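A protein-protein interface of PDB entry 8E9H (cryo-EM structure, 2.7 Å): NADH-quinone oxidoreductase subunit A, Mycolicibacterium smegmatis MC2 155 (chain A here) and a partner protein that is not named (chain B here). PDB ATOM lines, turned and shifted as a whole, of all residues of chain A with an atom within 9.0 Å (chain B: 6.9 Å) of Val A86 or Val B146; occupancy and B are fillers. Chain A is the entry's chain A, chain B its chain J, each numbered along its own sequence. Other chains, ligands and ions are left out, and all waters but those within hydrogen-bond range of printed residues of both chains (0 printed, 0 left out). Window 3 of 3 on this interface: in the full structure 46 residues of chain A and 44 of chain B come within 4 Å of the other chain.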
ATOM      1  N   VAL A  79      22.740 -28.165  -1.523  1.00  0.00           N
ATOM      2  CA  VAL A  79      22.095 -28.302  -2.822  1.00  0.00           C
ATOM      3  C   VAL A  79      21.602 -26.963  -3.342  1.00  0.00           C
ATOM      4  O   VAL A  79      21.312 -26.834  -4.534  1.00  0.00           O
ATOM      5  CB  VAL A  79      20.940 -29.318  -2.753  1.00  0.00           C
ATOM      6  CG1 VAL A  79      21.488 -30.731  -2.706  1.00  0.00           C
ATOM      7  CG2 VAL A  79      20.076 -29.058  -1.547  1.00  0.00           C
ATOM      8  N   PHE A  80      21.492 -25.955  -2.477  1.00  0.00           N
ATOM      9  CA  PHE A  80      21.184 -24.615  -2.956  1.00  0.00           C
ATOM     10  C   PHE A  80      22.266 -24.080  -3.877  1.00  0.00           C
ATOM     11  O   PHE A  80      21.993 -23.186  -4.683  1.00  0.00           O
ATOM     12  CB  PHE A  80      21.007 -23.657  -1.780  1.00  0.00           C
ATOM     13  CG  PHE A  80      19.615 -23.620  -1.230  1.00  0.00           C
ATOM     14  CD1 PHE A  80      18.560 -23.183  -2.009  1.00  0.00           C
ATOM     15  CD2 PHE A  80      19.362 -24.010   0.071  1.00  0.00           C
ATOM     16  CE1 PHE A  80      17.281 -23.144  -1.503  1.00  0.00           C
ATOM     17  CE2 PHE A  80      18.084 -23.972   0.581  1.00  0.00           C
ATOM     18  CZ  PHE A  80      17.043 -23.539  -0.206  1.00  0.00           C
ATOM     19  N   LEU A  81      23.487 -24.604  -3.779  1.00  0.00           N
ATOM     20  CA  LEU A  81      24.578 -24.082  -4.589  1.00  0.00           C
ATOM     21  C   LEU A  81      24.418 -24.448  -6.058  1.00  0.00           C
ATOM     22  O   LEU A  81      24.780 -23.655  -6.933  1.00  0.00           O
ATOM     23  CB  LEU A  81      25.912 -24.602  -4.059  1.00  0.00           C
ATOM     24  CG  LEU A  81      26.212 -24.243  -2.604  1.00  0.00           C
ATOM     25  CD1 LEU A  81      27.283 -25.149  -2.040  1.00  0.00           C
ATOM     26  CD2 LEU A  81      26.628 -22.796  -2.490  1.00  0.00           C
ATOM     27  N   TYR A  82      23.881 -25.639  -6.351  1.00  0.00           N
ATOM     28  CA  TYR A  82      23.830 -26.090  -7.742  1.00  0.00           C
ATOM     29  C   TYR A  82      23.039 -25.133  -8.619  1.00  0.00           C
ATOM     30  O   TYR A  82      23.564 -24.689  -9.656  1.00  0.00           O
ATOM     31  CB  TYR A  82      23.265 -27.507  -7.807  1.00  0.00           C
ATOM     32  CG  TYR A  82      24.029 -28.498  -6.971  1.00  0.00           C
ATOM     33  CD1 TYR A  82      25.411 -28.481  -6.933  1.00  0.00           C
ATOM     34  CD2 TYR A  82      23.364 -29.445  -6.214  1.00  0.00           C
ATOM     35  CE1 TYR A  82      26.107 -29.383  -6.170  1.00  0.00           C
ATOM     36  CE2 TYR A  82      24.053 -30.348  -5.449  1.00  0.00           C
ATOM     37  CZ  TYR A  82      25.422 -30.314  -5.430  1.00  0.00           C
ATOM     38  OH  TYR A  82      26.107 -31.220  -4.664  1.00  0.00           O
ATOM     39  N   PRO A  83      21.793 -24.781  -8.295  1.00  0.00           N
ATOM     40  CA  PRO A  83      21.099 -23.793  -9.132  1.00  0.00           C
ATOM     41  C   PRO A  83      21.817 -22.463  -9.153  1.00  0.00           C
ATOM     42  O   PRO A  83      21.833 -21.776 -10.181  1.00  0.00           O
ATOM     43  CB  PRO A  83      19.714 -23.700  -8.484  1.00  0.00           C
ATOM     44  CG  PRO A  83      19.925 -24.112  -7.086  1.00  0.00           C
ATOM     45  CD  PRO A  83      20.998 -25.150  -7.115  1.00  0.00           C
ATOM     46  N   TRP A  84      22.426 -22.083  -8.034  1.00  0.00           N
ATOM     47  CA  TRP A  84      23.223 -20.865  -7.999  1.00  0.00           C
ATOM     48  C   TRP A  84      24.426 -20.978  -8.922  1.00  0.00           C
ATOM     49  O   TRP A  84      24.737 -20.047  -9.673  1.00  0.00           O
ATOM     50  CB  TRP A  84      23.669 -20.592  -6.569  1.00  0.00           C
ATOM     51  CG  TRP A  84      24.617 -19.472  -6.441  1.00  0.00           C
ATOM     52  CD1 TRP A  84      24.343 -18.148  -6.571  1.00  0.00           C
ATOM     53  CD2 TRP A  84      26.007 -19.570  -6.141  1.00  0.00           C
ATOM     54  NE1 TRP A  84      25.481 -17.409  -6.373  1.00  0.00           N
ATOM     55  CE2 TRP A  84      26.517 -18.262  -6.104  1.00  0.00           C
ATOM     56  CE3 TRP A  84      26.870 -20.637  -5.894  1.00  0.00           C
ATOM     57  CZ2 TRP A  84      27.851 -17.993  -5.838  1.00  0.00           C
ATOM     58  CZ3 TRP A  84      28.189 -20.369  -5.629  1.00  0.00           C
ATOM     59  CH2 TRP A  84      28.668 -19.061  -5.602  1.00  0.00           C
ATOM     60  N   ALA A  85      25.115 -22.116  -8.879  1.00  0.00           N
ATOM     61  CA  ALA A  85      26.318 -22.277  -9.685  1.00  0.00           C
ATOM     62  C   ALA A  85      25.990 -22.253 -11.170  1.00  0.00           C
ATOM     63  O   ALA A  85      26.641 -21.555 -11.953  1.00  0.00           O
ATOM     64  CB  ALA A  85      27.024 -23.578  -9.310  1.00  0.00           C
ATOM     65  N   VAL A  86      24.968 -23.005 -11.578  1.00  0.00           N
ATOM     66  CA  VAL A  86      24.655 -23.092 -12.999  1.00  0.00           C
ATOM     67  C   VAL A  86      24.219 -21.739 -13.536  1.00  0.00           C
ATOM     68  O   VAL A  86      24.601 -21.352 -14.646  1.00  0.00           O
ATOM     69  CB  VAL A  86      23.583 -24.167 -13.254  1.00  0.00           C
ATOM     70  CG1 VAL A  86      24.061 -25.519 -12.767  1.00  0.00           C
ATOM     71  CG2 VAL A  86      22.277 -23.784 -12.592  1.00  0.00           C
ATOM     72  N   ALA A  87      23.422 -21.000 -12.772  1.00  0.00           N
ATOM     73  CA  ALA A  87      22.937 -19.696 -13.198  1.00  0.00           C
ATOM     74  C   ALA A  87      23.846 -18.556 -12.771  1.00  0.00           C
ATOM     75  O   ALA A  87      23.447 -17.394 -12.885  1.00  0.00           O
ATOM     76  CB  ALA A  87      21.532 -19.455 -12.640  1.00  0.00           C
ATOM     77  N   PHE A  88      25.053 -18.857 -12.293  1.00  0.00           N
ATOM     78  CA  PHE A  88      25.909 -17.829 -11.711  1.00  0.00           C
ATOM     79  C   PHE A  88      26.066 -16.635 -12.640  1.00  0.00           C
ATOM     80  O   PHE A  88      25.904 -15.484 -12.224  1.00  0.00           O
ATOM     81  CB  PHE A  88      27.270 -18.428 -11.375  1.00  0.00           C
ATOM     82  CG  PHE A  88      28.220 -17.455 -10.754  1.00  0.00           C
ATOM     83  CD1 PHE A  88      29.111 -16.747 -11.535  1.00  0.00           C
ATOM     84  CD2 PHE A  88      28.220 -17.242  -9.390  1.00  0.00           C
ATOM     85  CE1 PHE A  88      29.986 -15.852 -10.968  1.00  0.00           C
ATOM     86  CE2 PHE A  88      29.094 -16.349  -8.819  1.00  0.00           C
ATOM     87  CZ  PHE A  88      29.977 -15.651  -9.609  1.00  0.00           C
ATOM     88  N   ASP A  89      26.389 -16.890 -13.906  1.00  0.00           N
ATOM     89  CA  ASP A  89      26.604 -15.788 -14.835  1.00  0.00           C
ATOM     90  C   ASP A  89      25.334 -14.970 -15.021  1.00  0.00           C
ATOM     91  O   ASP A  89      25.382 -13.736 -15.062  1.00  0.00           O
ATOM     92  CB  ASP A  89      27.095 -16.327 -16.176  1.00  0.00           C
ATOM     93  CG  ASP A  89      28.357 -17.152 -16.043  1.00  0.00           C
ATOM     94  OD1 ASP A  89      29.311 -16.680 -15.393  1.00  0.00           O
ATOM     95  OD2 ASP A  89      28.392 -18.276 -16.583  1.00  0.00           O
ATOM     96  N   SER A  90      24.187 -15.640 -15.125  1.00  0.00           N
ATOM     97  CA  SER A  90      22.947 -14.934 -15.424  1.00  0.00           C
ATOM     98  C   SER A  90      22.447 -14.128 -14.235  1.00  0.00           C
ATOM     99  O   SER A  90      21.755 -13.122 -14.422  1.00  0.00           O
ATOM    100  CB  SER A  90      21.877 -15.930 -15.866  1.00  0.00           C
ATOM    101  OG  SER A  90      22.367 -16.775 -16.891  1.00  0.00           O
ATOM    102  N   LEU A  91      22.778 -14.542 -13.014  1.00  0.00           N
ATOM    103  CA  LEU A  91      22.217 -13.881 -11.841  1.00  0.00           C
ATOM    104  C   LEU A  91      22.820 -12.498 -11.633  1.00  0.00           C
ATOM    105  O   LEU A  91      22.100 -11.495 -11.628  1.00  0.00           O
ATOM    106  CB  LEU A  91      22.431 -14.744 -10.601  1.00  0.00           C
ATOM    107  CG  LEU A  91      21.683 -16.076 -10.584  1.00  0.00           C
ATOM    108  CD1 LEU A  91      22.173 -16.944  -9.446  1.00  0.00           C
ATOM    109  CD2 LEU A  91      20.189 -15.840 -10.472  1.00  0.00           C
ATOM    110  N   PRO B  67      13.270 -32.019 -13.239  1.00  0.00           N
ATOM    111  CA  PRO B  67      14.436 -32.911 -13.151  1.00  0.00           C
ATOM    112  C   PRO B  67      15.303 -32.632 -11.942  1.00  0.00           C
ATOM    113  O   PRO B  67      15.644 -33.553 -11.187  1.00  0.00           O
ATOM    114  CB  PRO B  67      15.179 -32.633 -14.464  1.00  0.00           C
ATOM    115  CG  PRO B  67      14.179 -31.996 -15.356  1.00  0.00           C
ATOM    116  CD  PRO B  67      13.302 -31.204 -14.460  1.00  0.00           C
ATOM    117  N   PHE B  68      15.671 -31.368 -11.738  1.00  0.00           N
ATOM    118  CA  PHE B  68      16.544 -31.028 -10.625  1.00  0.00           C
ATOM    119  C   PHE B  68      15.899 -31.398  -9.303  1.00  0.00           C
ATOM    120  O   PHE B  68      16.557 -31.930  -8.403  1.00  0.00           O
ATOM    121  CB  PHE B  68      16.875 -29.541 -10.654  1.00  0.00           C
ATOM    122  CG  PHE B  68      17.728 -29.099  -9.511  1.00  0.00           C
ATOM    123  CD1 PHE B  68      19.048 -29.493  -9.430  1.00  0.00           C
ATOM    124  CD2 PHE B  68      17.208 -28.305  -8.509  1.00  0.00           C
ATOM    125  CE1 PHE B  68      19.836 -29.093  -8.379  1.00  0.00           C
ATOM    126  CE2 PHE B  68      17.994 -27.904  -7.455  1.00  0.00           C
ATOM    127  CZ  PHE B  68      19.308 -28.301  -7.391  1.00  0.00           C
ATOM    128  N   LEU B  69      14.606 -31.116  -9.161  1.00  0.00           N
ATOM    129  CA  LEU B  69      13.926 -31.449  -7.919  1.00  0.00           C
ATOM    130  C   LEU B  69      13.963 -32.947  -7.666  1.00  0.00           C
ATOM    131  O   LEU B  69      14.224 -33.386  -6.545  1.00  0.00           O
ATOM    132  CB  LEU B  69      12.487 -30.948  -7.956  1.00  0.00           C
ATOM    133  CG  LEU B  69      11.767 -31.028  -6.614  1.00  0.00           C
ATOM    134  CD1 LEU B  69      12.254 -29.934  -5.689  1.00  0.00           C
ATOM    135  CD2 LEU B  69      10.275 -30.934  -6.807  1.00  0.00           C
ATOM    136  N   ASN B 141      10.511 -24.234 -18.248  1.00  0.00           N
ATOM    137  CA  ASN B 141      11.754 -24.984 -18.341  1.00  0.00           C
ATOM    138  C   ASN B 141      12.594 -24.577 -19.539  1.00  0.00           C
ATOM    139  O   ASN B 141      13.794 -24.870 -19.560  1.00  0.00           O
ATOM    140  CB  ASN B 141      11.462 -26.482 -18.408  1.00  0.00           C
ATOM    141  CG  ASN B 141      11.318 -27.107 -17.039  1.00  0.00           C
ATOM    142  OD1 ASN B 141      11.759 -26.549 -16.037  1.00  0.00           O
ATOM    143  ND2 ASN B 141      10.699 -28.277 -16.987  1.00  0.00           N
ATOM    144  N   GLY B 143      15.085 -22.597 -21.512  1.00  0.00           N
ATOM    145  CA  GLY B 143      16.198 -21.919 -20.888  1.00  0.00           C
ATOM    146  C   GLY B 143      16.749 -22.620 -19.669  1.00  0.00           C
ATOM    147  O   GLY B 143      17.518 -22.010 -18.918  1.00  0.00           O
ATOM    148  N   GLY B 144      16.371 -23.874 -19.442  1.00  0.00           N
ATOM    149  CA  GLY B 144      16.929 -24.651 -18.354  1.00  0.00           C
ATOM    150  C   GLY B 144      16.066 -24.645 -17.113  1.00  0.00           C
ATOM    151  O   GLY B 144      15.708 -23.582 -16.601  1.00  0.00           O
ATOM    152  N   ASN B 145      15.722 -25.834 -16.621  1.00  0.00           N
ATOM    153  CA  ASN B 145      14.938 -25.925 -15.394  1.00  0.00           C
ATOM    154  C   ASN B 145      15.722 -25.383 -14.208  1.00  0.00           C
ATOM    155  O   ASN B 145      15.193 -24.617 -13.394  1.00  0.00           O
ATOM    156  CB  ASN B 145      14.525 -27.375 -15.150  1.00  0.00           C
ATOM    157  CG  ASN B 145      13.733 -27.544 -13.878  1.00  0.00           C
ATOM    158  OD1 ASN B 145      14.137 -28.273 -12.975  1.00  0.00           O
ATOM    159  ND2 ASN B 145      12.596 -26.872 -13.799  1.00  0.00           N
ATOM    160  N   VAL B 146      16.994 -25.765 -14.097  1.00  0.00           N
ATOM    161  CA  VAL B 146      17.803 -25.296 -12.977  1.00  0.00           C
ATOM    162  C   VAL B 146      17.994 -23.791 -13.055  1.00  0.00           C
ATOM    163  O   VAL B 146      18.011 -23.104 -12.030  1.00  0.00           O
ATOM    164  CB  VAL B 146      19.157 -26.029 -12.932  1.00  0.00           C
ATOM    165  CG1 VAL B 146      18.965 -27.474 -12.529  1.00  0.00           C
ATOM    166  CG2 VAL B 146      19.889 -25.920 -14.259  1.00  0.00           C
ATOM    167  N   GLU B 147      18.150 -23.248 -14.263  1.00  0.00           N
ATOM    168  CA  GLU B 147      18.297 -21.804 -14.394  1.00  0.00           C
ATOM    169  C   GLU B 147      17.031 -21.076 -13.959  1.00  0.00           C
ATOM    170  O   GLU B 147      17.106 -20.047 -13.281  1.00  0.00           O
ATOM    171  CB  GLU B 147      18.662 -21.443 -15.829  1.00  0.00           C
ATOM    172  CG  GLU B 147      20.093 -21.783 -16.185  1.00  0.00           C
ATOM    173  CD  GLU B 147      20.224 -23.159 -16.789  1.00  0.00           C
ATOM    174  OE1 GLU B 147      19.406 -24.034 -16.444  1.00  0.00           O
ATOM    175  OE2 GLU B 147      21.148 -23.369 -17.602  1.00  0.00           O
ATOM    176  N   GLY B 148      15.861 -21.588 -14.338  1.00  0.00           N
ATOM    177  CA  GLY B 148      14.626 -20.980 -13.874  1.00  0.00           C
ATOM    178  C   GLY B 148      14.478 -21.057 -12.367  1.00  0.00           C
ATOM    179  O   GLY B 148      14.071 -20.087 -11.719  1.00  0.00           O
ATOM    180  N   LEU B 149      14.813 -22.211 -11.788  1.00  0.00           N
ATOM    181  CA  LEU B 149      14.759 -22.343 -10.337  1.00  0.00           C
ATOM    182  C   LEU B 149      15.703 -21.360  -9.667  1.00  0.00           C
ATOM    183  O   LEU B 149      15.358 -20.757  -8.646  1.00  0.00           O
ATOM    184  CB  LEU B 149      15.108 -23.770  -9.926  1.00  0.00           C
ATOM    185  CG  LEU B 149      14.073 -24.837 -10.262  1.00  0.00           C
ATOM    186  CD1 LEU B 149      14.669 -26.214 -10.062  1.00  0.00           C
ATOM    187  CD2 LEU B 149      12.839 -24.662  -9.412  1.00  0.00           C
ATOM    188  N   ALA B 150      16.905 -21.195 -10.214  1.00  0.00           N
ATOM    189  CA  ALA B 150      17.849 -20.243  -9.646  1.00  0.00           C
ATOM    190  C   ALA B 150      17.314 -18.824  -9.742  1.00  0.00           C
ATOM    191  O   ALA B 150      17.421 -18.045  -8.789  1.00  0.00           O
ATOM    192  CB  ALA B 150      19.194 -20.355 -10.359  1.00  0.00           C
ATOM    193  N   ALA B 151      16.729 -18.469 -10.883  1.00  0.00           N
ATOM    194  CA  ALA B 151      16.186 -17.126 -11.036  1.00  0.00           C
ATOM    195  C   ALA B 151      15.100 -16.861 -10.005  1.00  0.00           C
ATOM    196  O   ALA B 151      15.062 -15.789  -9.394  1.00  0.00           O
ATOM    197  CB  ALA B 151      15.641 -16.939 -12.449  1.00  0.00           C
ATOM    198  N   LEU B 152      14.212 -17.831  -9.793  1.00  0.00           N
ATOM    199  CA  LEU B 152      13.154 -17.640  -8.806  1.00  0.00           C
ATOM    200  C   LEU B 152      13.722 -17.573  -7.394  1.00  0.00           C
ATOM    201  O   LEU B 152      13.367 -16.683  -6.614  1.00  0.00           O
ATOM    202  CB  LEU B 152      12.127 -18.764  -8.913  1.00  0.00           C
ATOM    203  CG  LEU B 152      10.902 -18.439  -9.761  1.00  0.00           C
ATOM    204  CD1 LEU B 152      11.316 -18.013 -11.155  1.00  0.00           C
ATOM    205  CD2 LEU B 152       9.984 -19.640  -9.818  1.00  0.00           C
ATOM    206  N   ILE B 153      14.611 -18.503  -7.050  1.00  0.00           N
ATOM    207  CA  ILE B 153      15.058 -18.634  -5.666  1.00  0.00           C
ATOM    208  C   ILE B 153      15.788 -17.378  -5.217  1.00  0.00           C
ATOM    209  O   ILE B 153      15.556 -16.862  -4.118  1.00  0.00           O
ATOM    210  CB  ILE B 153      15.947 -19.878  -5.504  1.00  0.00           C
ATOM    211  CG1 ILE B 153      15.105 -21.149  -5.578  1.00  0.00           C
ATOM    212  CG2 ILE B 153      16.693 -19.823  -4.186  1.00  0.00           C
ATOM    213  CD1 ILE B 153      15.914 -22.401  -5.816  1.00  0.00           C
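CZ of Phe B68 touches O of Val A79, at 3.8 Å.
CE1 of Phe B68 touches CB of Tyr A82, 3.8 Å away.
Pro A83 touches Phe B68.
CB of Pro A83 touches O of Val B146, 3.98 Å away.
Pro A83 touches Ala B150 (O to CB, 3.0 Å).
CG2 of Val B146 touches CG2 of Val A86, 3.6 Å away.
Ala B150 touches Ala A87.
Leu A91 touches Ala B150.
Printed residues of chain B within 4 Å of Tyr A82: Phe B68 (3.8 Å).
Printed residues of chain B within 4 Å of Pro A83: Phe B68, Val B146 and Ala B150.
Of chain B, only Val B146 comes within 4 Å of Val A86.
Asp A89 touches none of the printed residues of chain B.
Of the printed residues of chain B, Leu A91 touches Ala B150 (3.9 Å).
Of chain A, only Pro A83 (3.98 Å) and Val A86 (3.6 Å) come within 4 Å of Val B146.
Printed residues of chain A within 4 Å of Ala B150: Pro A83, Ala A87 and Leu A91.
Leu B152 touches none of the printed residues of chain A.
The nearest residue of chain A that does not touch Val B146 is Ala A87 (5.1 Å).
The nearest printed residue of chain B that does not touch Leu A91 is Ala B151 (4.2 Å).
Of the 13 printed residues of chain A, 6 touch a printed residue of chain B.
Along chain A the printed residues that touch a printed residue of chain B span positions 79 to 91.
Along chain B the printed residues that touch a printed residue of chain A span positions 68 to 150.
Among the printed residues, 8 pairs touch across the chains.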
